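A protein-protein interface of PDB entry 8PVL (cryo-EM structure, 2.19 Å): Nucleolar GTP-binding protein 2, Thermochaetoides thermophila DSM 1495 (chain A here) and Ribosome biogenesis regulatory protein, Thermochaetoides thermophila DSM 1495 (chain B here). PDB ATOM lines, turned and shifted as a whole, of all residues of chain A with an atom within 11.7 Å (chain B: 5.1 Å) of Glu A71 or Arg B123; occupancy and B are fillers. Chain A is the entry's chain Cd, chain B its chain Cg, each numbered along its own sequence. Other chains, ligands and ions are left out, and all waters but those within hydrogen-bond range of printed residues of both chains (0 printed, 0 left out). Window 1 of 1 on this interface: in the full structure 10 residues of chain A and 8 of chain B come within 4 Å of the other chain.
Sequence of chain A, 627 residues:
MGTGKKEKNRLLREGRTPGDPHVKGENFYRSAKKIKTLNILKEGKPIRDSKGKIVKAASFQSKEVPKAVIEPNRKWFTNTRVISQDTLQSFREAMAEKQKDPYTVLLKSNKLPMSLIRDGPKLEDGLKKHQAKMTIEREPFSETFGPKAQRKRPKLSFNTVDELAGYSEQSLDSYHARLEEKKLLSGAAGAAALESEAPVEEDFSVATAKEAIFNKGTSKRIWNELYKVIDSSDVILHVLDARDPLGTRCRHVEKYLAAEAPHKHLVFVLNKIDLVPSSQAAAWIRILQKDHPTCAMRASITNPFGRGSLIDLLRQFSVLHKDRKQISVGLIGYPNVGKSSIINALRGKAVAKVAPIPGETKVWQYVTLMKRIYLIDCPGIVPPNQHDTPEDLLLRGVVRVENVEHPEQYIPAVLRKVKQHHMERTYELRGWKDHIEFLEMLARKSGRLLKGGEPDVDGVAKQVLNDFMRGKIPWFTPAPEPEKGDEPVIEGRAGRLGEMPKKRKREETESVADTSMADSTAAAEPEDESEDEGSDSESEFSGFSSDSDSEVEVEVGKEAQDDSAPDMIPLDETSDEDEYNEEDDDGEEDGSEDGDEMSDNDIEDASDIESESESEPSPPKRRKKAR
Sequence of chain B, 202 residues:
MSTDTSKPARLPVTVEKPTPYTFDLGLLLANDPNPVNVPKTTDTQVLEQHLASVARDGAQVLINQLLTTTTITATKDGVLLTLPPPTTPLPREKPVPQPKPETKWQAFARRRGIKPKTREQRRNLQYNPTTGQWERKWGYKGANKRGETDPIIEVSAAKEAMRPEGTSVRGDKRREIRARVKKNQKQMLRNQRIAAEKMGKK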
ATOM      1  N   LYS A  67      -2.393   7.331  18.127  1.00  0.00           N
ATOM      2  CA  LYS A  67      -2.812   6.073  17.525  1.00  0.00           C
ATOM      3  C   LYS A  67      -2.253   4.929  18.360  1.00  0.00           C
ATOM      4  O   LYS A  67      -1.033   4.742  18.430  1.00  0.00           O
ATOM      5  CB  LYS A  67      -2.339   5.974  16.076  1.00  0.00           C
ATOM      6  CG  LYS A  67      -3.233   6.700  15.084  1.00  0.00           C
ATOM      7  CD  LYS A  67      -4.684   6.279  15.242  1.00  0.00           C
ATOM      8  CE  LYS A  67      -5.577   6.942  14.208  1.00  0.00           C
ATOM      9  NZ  LYS A  67      -5.327   6.424  12.837  1.00  0.00           N
ATOM     10  N   ALA A  68      -3.141   4.175  19.001  1.00  0.00           N
ATOM     11  CA  ALA A  68      -2.753   3.106  19.919  1.00  0.00           C
ATOM     12  C   ALA A  68      -2.903   1.779  19.183  1.00  0.00           C
ATOM     13  O   ALA A  68      -3.980   1.186  19.137  1.00  0.00           O
ATOM     14  CB  ALA A  68      -3.595   3.154  21.188  1.00  0.00           C
ATOM     15  N   VAL A  69      -1.801   1.308  18.609  1.00  0.00           N
ATOM     16  CA  VAL A  69      -1.794   0.119  17.769  1.00  0.00           C
ATOM     17  C   VAL A  69      -0.647  -0.785  18.193  1.00  0.00           C
ATOM     18  O   VAL A  69       0.466  -0.314  18.450  1.00  0.00           O
ATOM     19  CB  VAL A  69      -1.676   0.484  16.276  1.00  0.00           C
ATOM     20  CG1 VAL A  69      -3.043   0.777  15.699  1.00  0.00           C
ATOM     21  CG2 VAL A  69      -0.769   1.685  16.098  1.00  0.00           C
ATOM     22  N   ILE A  70      -0.924  -2.083  18.272  1.00  0.00           N
ATOM     23  CA  ILE A  70       0.088  -3.100  18.532  1.00  0.00           C
ATOM     24  C   ILE A  70       0.448  -3.755  17.209  1.00  0.00           C
ATOM     25  O   ILE A  70      -0.434  -4.227  16.482  1.00  0.00           O
ATOM     26  CB  ILE A  70      -0.411  -4.144  19.545  1.00  0.00           C
ATOM     27  CG1 ILE A  70      -0.897  -3.465  20.828  1.00  0.00           C
ATOM     28  CG2 ILE A  70       0.680  -5.169  19.842  1.00  0.00           C
ATOM     29  CD1 ILE A  70       0.216  -3.003  21.746  1.00  0.00           C
ATOM     30  N   GLU A  71       1.736  -3.781  16.889  1.00  0.00           N
ATOM     31  CA  GLU A  71       2.155  -4.372  15.631  1.00  0.00           C
ATOM     32  C   GLU A  71       2.158  -5.897  15.730  1.00  0.00           C
ATOM     33  O   GLU A  71       2.279  -6.456  16.824  1.00  0.00           O
ATOM     34  CB  GLU A  71       3.544  -3.866  15.235  1.00  0.00           C
ATOM     35  CG  GLU A  71       4.720  -4.666  15.779  1.00  0.00           C
ATOM     36  CD  GLU A  71       5.132  -4.242  17.175  1.00  0.00           C
ATOM     37  OE1 GLU A  71       4.487  -3.336  17.742  1.00  0.00           O
ATOM     38  OE2 GLU A  71       6.105  -4.813  17.707  1.00  0.00           O
ATOM     39  N   PRO A  72       1.973  -6.592  14.610  1.00  0.00           N
ATOM     40  CA  PRO A  72       2.178  -8.043  14.614  1.00  0.00           C
ATOM     41  C   PRO A  72       3.650  -8.378  14.790  1.00  0.00           C
ATOM     42  O   PRO A  72       4.523  -7.778  14.158  1.00  0.00           O
ATOM     43  CB  PRO A  72       1.658  -8.483  13.240  1.00  0.00           C
ATOM     44  CG  PRO A  72       1.670  -7.250  12.409  1.00  0.00           C
ATOM     45  CD  PRO A  72       1.384  -6.123  13.345  1.00  0.00           C
ATOM     46  N   ASN A  73       3.918  -9.343  15.662  1.00  0.00           N
ATOM     47  CA  ASN A  73       5.286  -9.696  16.006  1.00  0.00           C
ATOM     48  C   ASN A  73       5.306 -11.129  16.512  1.00  0.00           C
ATOM     49  O   ASN A  73       4.451 -11.520  17.308  1.00  0.00           O
ATOM     50  CB  ASN A  73       5.855  -8.745  17.066  1.00  0.00           C
ATOM     51  CG  ASN A  73       7.370  -8.728  17.093  1.00  0.00           C
ATOM     52  OD1 ASN A  73       8.020  -9.770  17.045  1.00  0.00           O
ATOM     53  ND2 ASN A  73       7.940  -7.535  17.179  1.00  0.00           N
ATOM     54  N   ARG A  74       6.289 -11.901  16.045  1.00  0.00           N
ATOM     55  CA  ARG A  74       6.440 -13.278  16.497  1.00  0.00           C
ATOM     56  C   ARG A  74       6.845 -13.367  17.961  1.00  0.00           C
ATOM     57  O   ARG A  74       6.656 -14.419  18.579  1.00  0.00           O
ATOM     58  CB  ARG A  74       7.468 -14.005  15.628  1.00  0.00           C
ATOM     59  N   LYS A  75       7.392 -12.288  18.530  1.00  0.00           N
ATOM     60  CA  LYS A  75       7.821 -12.299  19.922  1.00  0.00           C
ATOM     61  C   LYS A  75       6.655 -12.373  20.902  1.00  0.00           C
ATOM     62  O   LYS A  75       6.870 -12.739  22.062  1.00  0.00           O
ATOM     63  CB  LYS A  75       8.674 -11.062  20.217  1.00  0.00           C
ATOM     64  CG  LYS A  75       7.875  -9.801  20.510  1.00  0.00           C
ATOM     65  CD  LYS A  75       8.650  -8.825  21.379  1.00  0.00           C
ATOM     66  CE  LYS A  75       9.649  -8.028  20.563  1.00  0.00           C
ATOM     67  NZ  LYS A  75      10.172  -6.859  21.319  1.00  0.00           N
ATOM     68  N   TRP A  76       5.432 -12.043  20.472  1.00  0.00           N
ATOM     69  CA  TRP A  76       4.292 -12.112  21.378  1.00  0.00           C
ATOM     70  C   TRP A  76       3.889 -13.542  21.703  1.00  0.00           C
ATOM     71  O   TRP A  76       3.205 -13.767  22.706  1.00  0.00           O
ATOM     72  CB  TRP A  76       3.073 -11.387  20.795  1.00  0.00           C
ATOM     73  CG  TRP A  76       3.279  -9.976  20.295  1.00  0.00           C
ATOM     74  CD1 TRP A  76       2.866  -9.480  19.094  1.00  0.00           C
ATOM     75  CD2 TRP A  76       3.901  -8.879  20.985  1.00  0.00           C
ATOM     76  NE1 TRP A  76       3.200  -8.156  18.985  1.00  0.00           N
ATOM     77  CE2 TRP A  76       3.839  -7.763  20.129  1.00  0.00           C
ATOM     78  CE3 TRP A  76       4.509  -8.733  22.237  1.00  0.00           C
ATOM     79  CZ2 TRP A  76       4.362  -6.522  20.482  1.00  0.00           C
ATOM     80  CZ3 TRP A  76       5.028  -7.502  22.582  1.00  0.00           C
ATOM     81  CH2 TRP A  76       4.949  -6.413  21.709  1.00  0.00           C
ATOM     82  N   PHE A  77       4.295 -14.511  20.884  1.00  0.00           N
ATOM     83  CA  PHE A  77       3.805 -15.877  20.990  1.00  0.00           C
ATOM     84  C   PHE A  77       4.893 -16.853  21.420  1.00  0.00           C
ATOM     85  O   PHE A  77       4.758 -18.061  21.206  1.00  0.00           O
ATOM     86  CB  PHE A  77       3.185 -16.307  19.660  1.00  0.00           C
ATOM     87  CG  PHE A  77       2.040 -15.437  19.224  1.00  0.00           C
ATOM     88  CD1 PHE A  77       0.750 -15.704  19.650  1.00  0.00           C
ATOM     89  CD2 PHE A  77       2.256 -14.342  18.402  1.00  0.00           C
ATOM     90  CE1 PHE A  77      -0.302 -14.902  19.257  1.00  0.00           C
ATOM     91  CE2 PHE A  77       1.206 -13.535  18.012  1.00  0.00           C
ATOM     92  CZ  PHE A  77      -0.074 -13.817  18.437  1.00  0.00           C
ATOM     93  N   ARG B 119      16.227   0.154  21.890  1.00  0.00           N
ATOM     94  CA  ARG B 119      16.074  -0.717  20.732  1.00  0.00           C
ATOM     95  C   ARG B 119      14.645  -0.704  20.206  1.00  0.00           C
ATOM     96  O   ARG B 119      14.431  -0.876  19.002  1.00  0.00           O
ATOM     97  CB  ARG B 119      16.512  -2.136  21.087  1.00  0.00           C
ATOM     98  CG  ARG B 119      17.961  -2.224  21.541  1.00  0.00           C
ATOM     99  CD  ARG B 119      18.354  -3.642  21.903  1.00  0.00           C
ATOM    100  NE  ARG B 119      18.429  -4.496  20.725  1.00  0.00           N
ATOM    101  CZ  ARG B 119      19.549  -4.787  20.080  1.00  0.00           C
ATOM    102  NH1 ARG B 119      20.720  -4.323  20.484  1.00  0.00           N
ATOM    103  NH2 ARG B 119      19.495  -5.563  19.002  1.00  0.00           N
ATOM    104  N   GLU B 120      13.662  -0.501  21.086  1.00  0.00           N
ATOM    105  CA  GLU B 120      12.291  -0.305  20.630  1.00  0.00           C
ATOM    106  C   GLU B 120      12.125   1.046  19.945  1.00  0.00           C
ATOM    107  O   GLU B 120      11.340   1.178  19.000  1.00  0.00           O
ATOM    108  CB  GLU B 120      11.325  -0.431  21.807  1.00  0.00           C
ATOM    109  CG  GLU B 120       9.867  -0.622  21.413  1.00  0.00           C
ATOM    110  CD  GLU B 120       9.677  -1.632  20.294  1.00  0.00           C
ATOM    111  OE1 GLU B 120      10.155  -2.779  20.431  1.00  0.00           O
ATOM    112  OE2 GLU B 120       9.047  -1.278  19.276  1.00  0.00           O
ATOM    113  N   GLN B 121      12.853   2.060  20.415  1.00  0.00           N
ATOM    114  CA  GLN B 121      12.756   3.395  19.833  1.00  0.00           C
ATOM    115  C   GLN B 121      13.349   3.448  18.431  1.00  0.00           C
ATOM    116  O   GLN B 121      12.825   4.158  17.567  1.00  0.00           O
ATOM    117  CB  GLN B 121      13.448   4.404  20.751  1.00  0.00           C
ATOM    118  CG  GLN B 121      13.452   5.842  20.273  1.00  0.00           C
ATOM    119  CD  GLN B 121      14.168   6.759  21.242  1.00  0.00           C
ATOM    120  OE1 GLN B 121      14.600   6.334  22.313  1.00  0.00           O
ATOM    121  NE2 GLN B 121      14.300   8.026  20.872  1.00  0.00           N
ATOM    122  N   ARG B 122      14.424   2.701  18.179  1.00  0.00           N
ATOM    123  CA  ARG B 122      15.109   2.769  16.894  1.00  0.00           C
ATOM    124  C   ARG B 122      14.641   1.706  15.899  1.00  0.00           C
ATOM    125  O   ARG B 122      15.324   1.473  14.896  1.00  0.00           O
ATOM    126  CB  ARG B 122      16.623   2.668  17.094  1.00  0.00           C
ATOM    127  CG  ARG B 122      17.100   1.316  17.584  1.00  0.00           C
ATOM    128  CD  ARG B 122      18.474   1.413  18.209  1.00  0.00           C
ATOM    129  NE  ARG B 122      19.101   0.101  18.314  1.00  0.00           N
ATOM    130  CZ  ARG B 122      20.127  -0.175  19.105  1.00  0.00           C
ATOM    131  NH1 ARG B 122      20.671   0.748  19.880  1.00  0.00           N
ATOM    132  NH2 ARG B 122      20.618  -1.410  19.121  1.00  0.00           N
ATOM    133  N   ARG B 123      13.498   1.068  16.143  1.00  0.00           N
ATOM    134  CA  ARG B 123      13.009   0.036  15.235  1.00  0.00           C
ATOM    135  C   ARG B 123      12.582   0.631  13.897  1.00  0.00           C
ATOM    136  O   ARG B 123      12.052   1.742  13.823  1.00  0.00           O
ATOM    137  CB  ARG B 123      11.834  -0.717  15.856  1.00  0.00           C
ATOM    138  CG  ARG B 123      12.233  -1.835  16.794  1.00  0.00           C
ATOM    139  CD  ARG B 123      11.072  -2.778  17.041  1.00  0.00           C
ATOM    140  NE  ARG B 123      10.669  -3.472  15.823  1.00  0.00           N
ATOM    141  CZ  ARG B 123       9.498  -4.068  15.653  1.00  0.00           C
ATOM    142  NH1 ARG B 123       8.572  -4.053  16.597  1.00  0.00           N
ATOM    143  NH2 ARG B 123       9.248  -4.692  14.506  1.00  0.00           N
ATOM    144  N   ASN B 124      12.815  -0.134  12.830  1.00  0.00           N
ATOM    145  CA  ASN B 124      12.468   0.287  11.471  1.00  0.00           C
ATOM    146  C   ASN B 124      11.018  -0.097  11.173  1.00  0.00           C
ATOM    147  O   ASN B 124      10.713  -0.933  10.322  1.00  0.00           O
ATOM    148  CB  ASN B 124      13.432  -0.327  10.464  1.00  0.00           C
ATOM    149  CG  ASN B 124      13.277   0.256   9.075  1.00  0.00           C
ATOM    150  OD1 ASN B 124      12.694   1.325   8.901  1.00  0.00           O
ATOM    151  ND2 ASN B 124      13.789  -0.449   8.076  1.00  0.00           N
ATOM    152  N   LEU B 125      10.113   0.543  11.908  1.00  0.00           N
ATOM    153  CA  LEU B 125       8.692   0.264  11.787  1.00  0.00           C
ATOM    154  C   LEU B 125       7.912   1.453  12.323  1.00  0.00           C
ATOM    155  O   LEU B 125       8.284   2.034  13.345  1.00  0.00           O
ATOM    156  CB  LEU B 125       8.306  -1.010  12.546  1.00  0.00           C
ATOM    157  CG  LEU B 125       6.981  -1.658  12.149  1.00  0.00           C
ATOM    158  CD1 LEU B 125       7.032  -2.141  10.708  1.00  0.00           C
ATOM    159  CD2 LEU B 125       6.639  -2.802  13.088  1.00  0.00           C
ATOM    160  N   TRP B 134       1.289  -0.915   8.814  1.00  0.00           N
ATOM    161  CA  TRP B 134       2.644  -0.846   9.347  1.00  0.00           C
ATOM    162  C   TRP B 134       3.639  -0.822   8.195  1.00  0.00           C
ATOM    163  O   TRP B 134       3.542  -1.632   7.268  1.00  0.00           O
ATOM    164  CB  TRP B 134       2.923  -2.026  10.278  1.00  0.00           C
ATOM    165  CG  TRP B 134       2.158  -1.952  11.560  1.00  0.00           C
ATOM    166  CD1 TRP B 134       0.971  -2.559  11.842  1.00  0.00           C
ATOM    167  CD2 TRP B 134       2.518  -1.212  12.732  1.00  0.00           C
ATOM    168  NE1 TRP B 134       0.573  -2.251  13.118  1.00  0.00           N
ATOM    169  CE2 TRP B 134       1.506  -1.426  13.686  1.00  0.00           C
ATOM    170  CE3 TRP B 134       3.601  -0.396  13.069  1.00  0.00           C
ATOM    171  CZ2 TRP B 134       1.543  -0.849  14.953  1.00  0.00           C
ATOM    172  CZ3 TRP B 134       3.635   0.174  14.327  1.00  0.00           C
ATOM    173  CH2 TRP B 134       2.613  -0.055  15.253  1.00  0.00           C
ATOM    174  N   LYS B 137      10.415   2.648   7.959  1.00  0.00           N
ATOM    175  CA  LYS B 137      10.812   4.044   7.817  1.00  0.00           C
ATOM    176  C   LYS B 137      11.841   4.224   6.709  1.00  0.00           C
ATOM    177  O   LYS B 137      11.783   5.203   5.957  1.00  0.00           O
ATOM    178  CB  LYS B 137      11.363   4.577   9.139  1.00  0.00           C
ATOM    179  CG  LYS B 137      10.426   4.427  10.322  1.00  0.00           C
ATOM    180  CD  LYS B 137      11.139   4.762  11.618  1.00  0.00           C
ATOM    181  CE  LYS B 137      10.178   4.791  12.792  1.00  0.00           C
ATOM    182  NZ  LYS B 137      10.899   4.914  14.088  1.00  0.00           N
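Of the 9 printed residues of chain B, 3 touch a printed residue of chain A.
Hydrophobic or aromatic side chains of chain A within 4 Å of the printed part of chain B: Val A69 and Pro A72.
Among the printed residues, Asp or Glu carboxylates within 4 Å of a Lys or Arg side-chain nitrogen of the other chain: Glu A71 with Arg B123 (2.8 Å).
Among the printed residues, merely in contact across the chains: Val A69 with Trp B134, Ile A70 with Trp B134, Glu A71 with Leu B125, Glu A71 with Trp B134, Pro A72 with Trp B134 and Asn A73 with Arg B123.
The guanidinium group (NH1) of Arg B123 is in salt-bridge range of the side-chain carboxylate (OE2) of Glu A71 (2.8 Å).
Printed residues of chain B within 4 Å of Val A69: Trp B134.
Of chain B, only Arg B123 (2.8 Å), Leu B125 (3.8 Å) and Trp B134 (3.5 Å) come within 4 Å of Glu A71.
No residue of chain A comes within 4 Å of Glu B120.
Arg B123 touches two residues of chain A.
No residue of chain A comes within 4 Å of Asn B124.
Of chain A, only Glu A71 comes within 4 Å of Leu B125.
Of the printed residues of chain A, Trp B134 touches Val A69 (3.6 Å), Ile A70 (3.8 Å), Glu A71 (3.5 Å) and Pro A72 (3.9 Å).
The nearest residue of chain B that does not touch Glu A71 is Glu B120 (4.9 Å).
The nearest residue of chain A that does not touch Arg B123 is Pro A72 (5.7 Å).
The nearest printed residue of chain B that does not touch Val A69 is Leu B125 (8.5 Å).
The side-chain carboxylate (OE2) of Glu A71 sits at hydrogen-bond distance from the side-chain amide nitrogen (ND2) of Asn A73.
O of Glu A71 is in hydrogen-bond range of NE1 of Trp A76 (2.9 Å).
OD1 of Asn A73 is in hydrogen-bond range of N of Lys A75.
The guanidinium group (NH1) of Arg B123 lies within salt-bridge range of the side-chain carboxylate (OE2) of Glu B120 (3.9 Å).
NZ of Lys B137 sits at hydrogen-bond distance from O of Arg B123 (3.4 Å).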
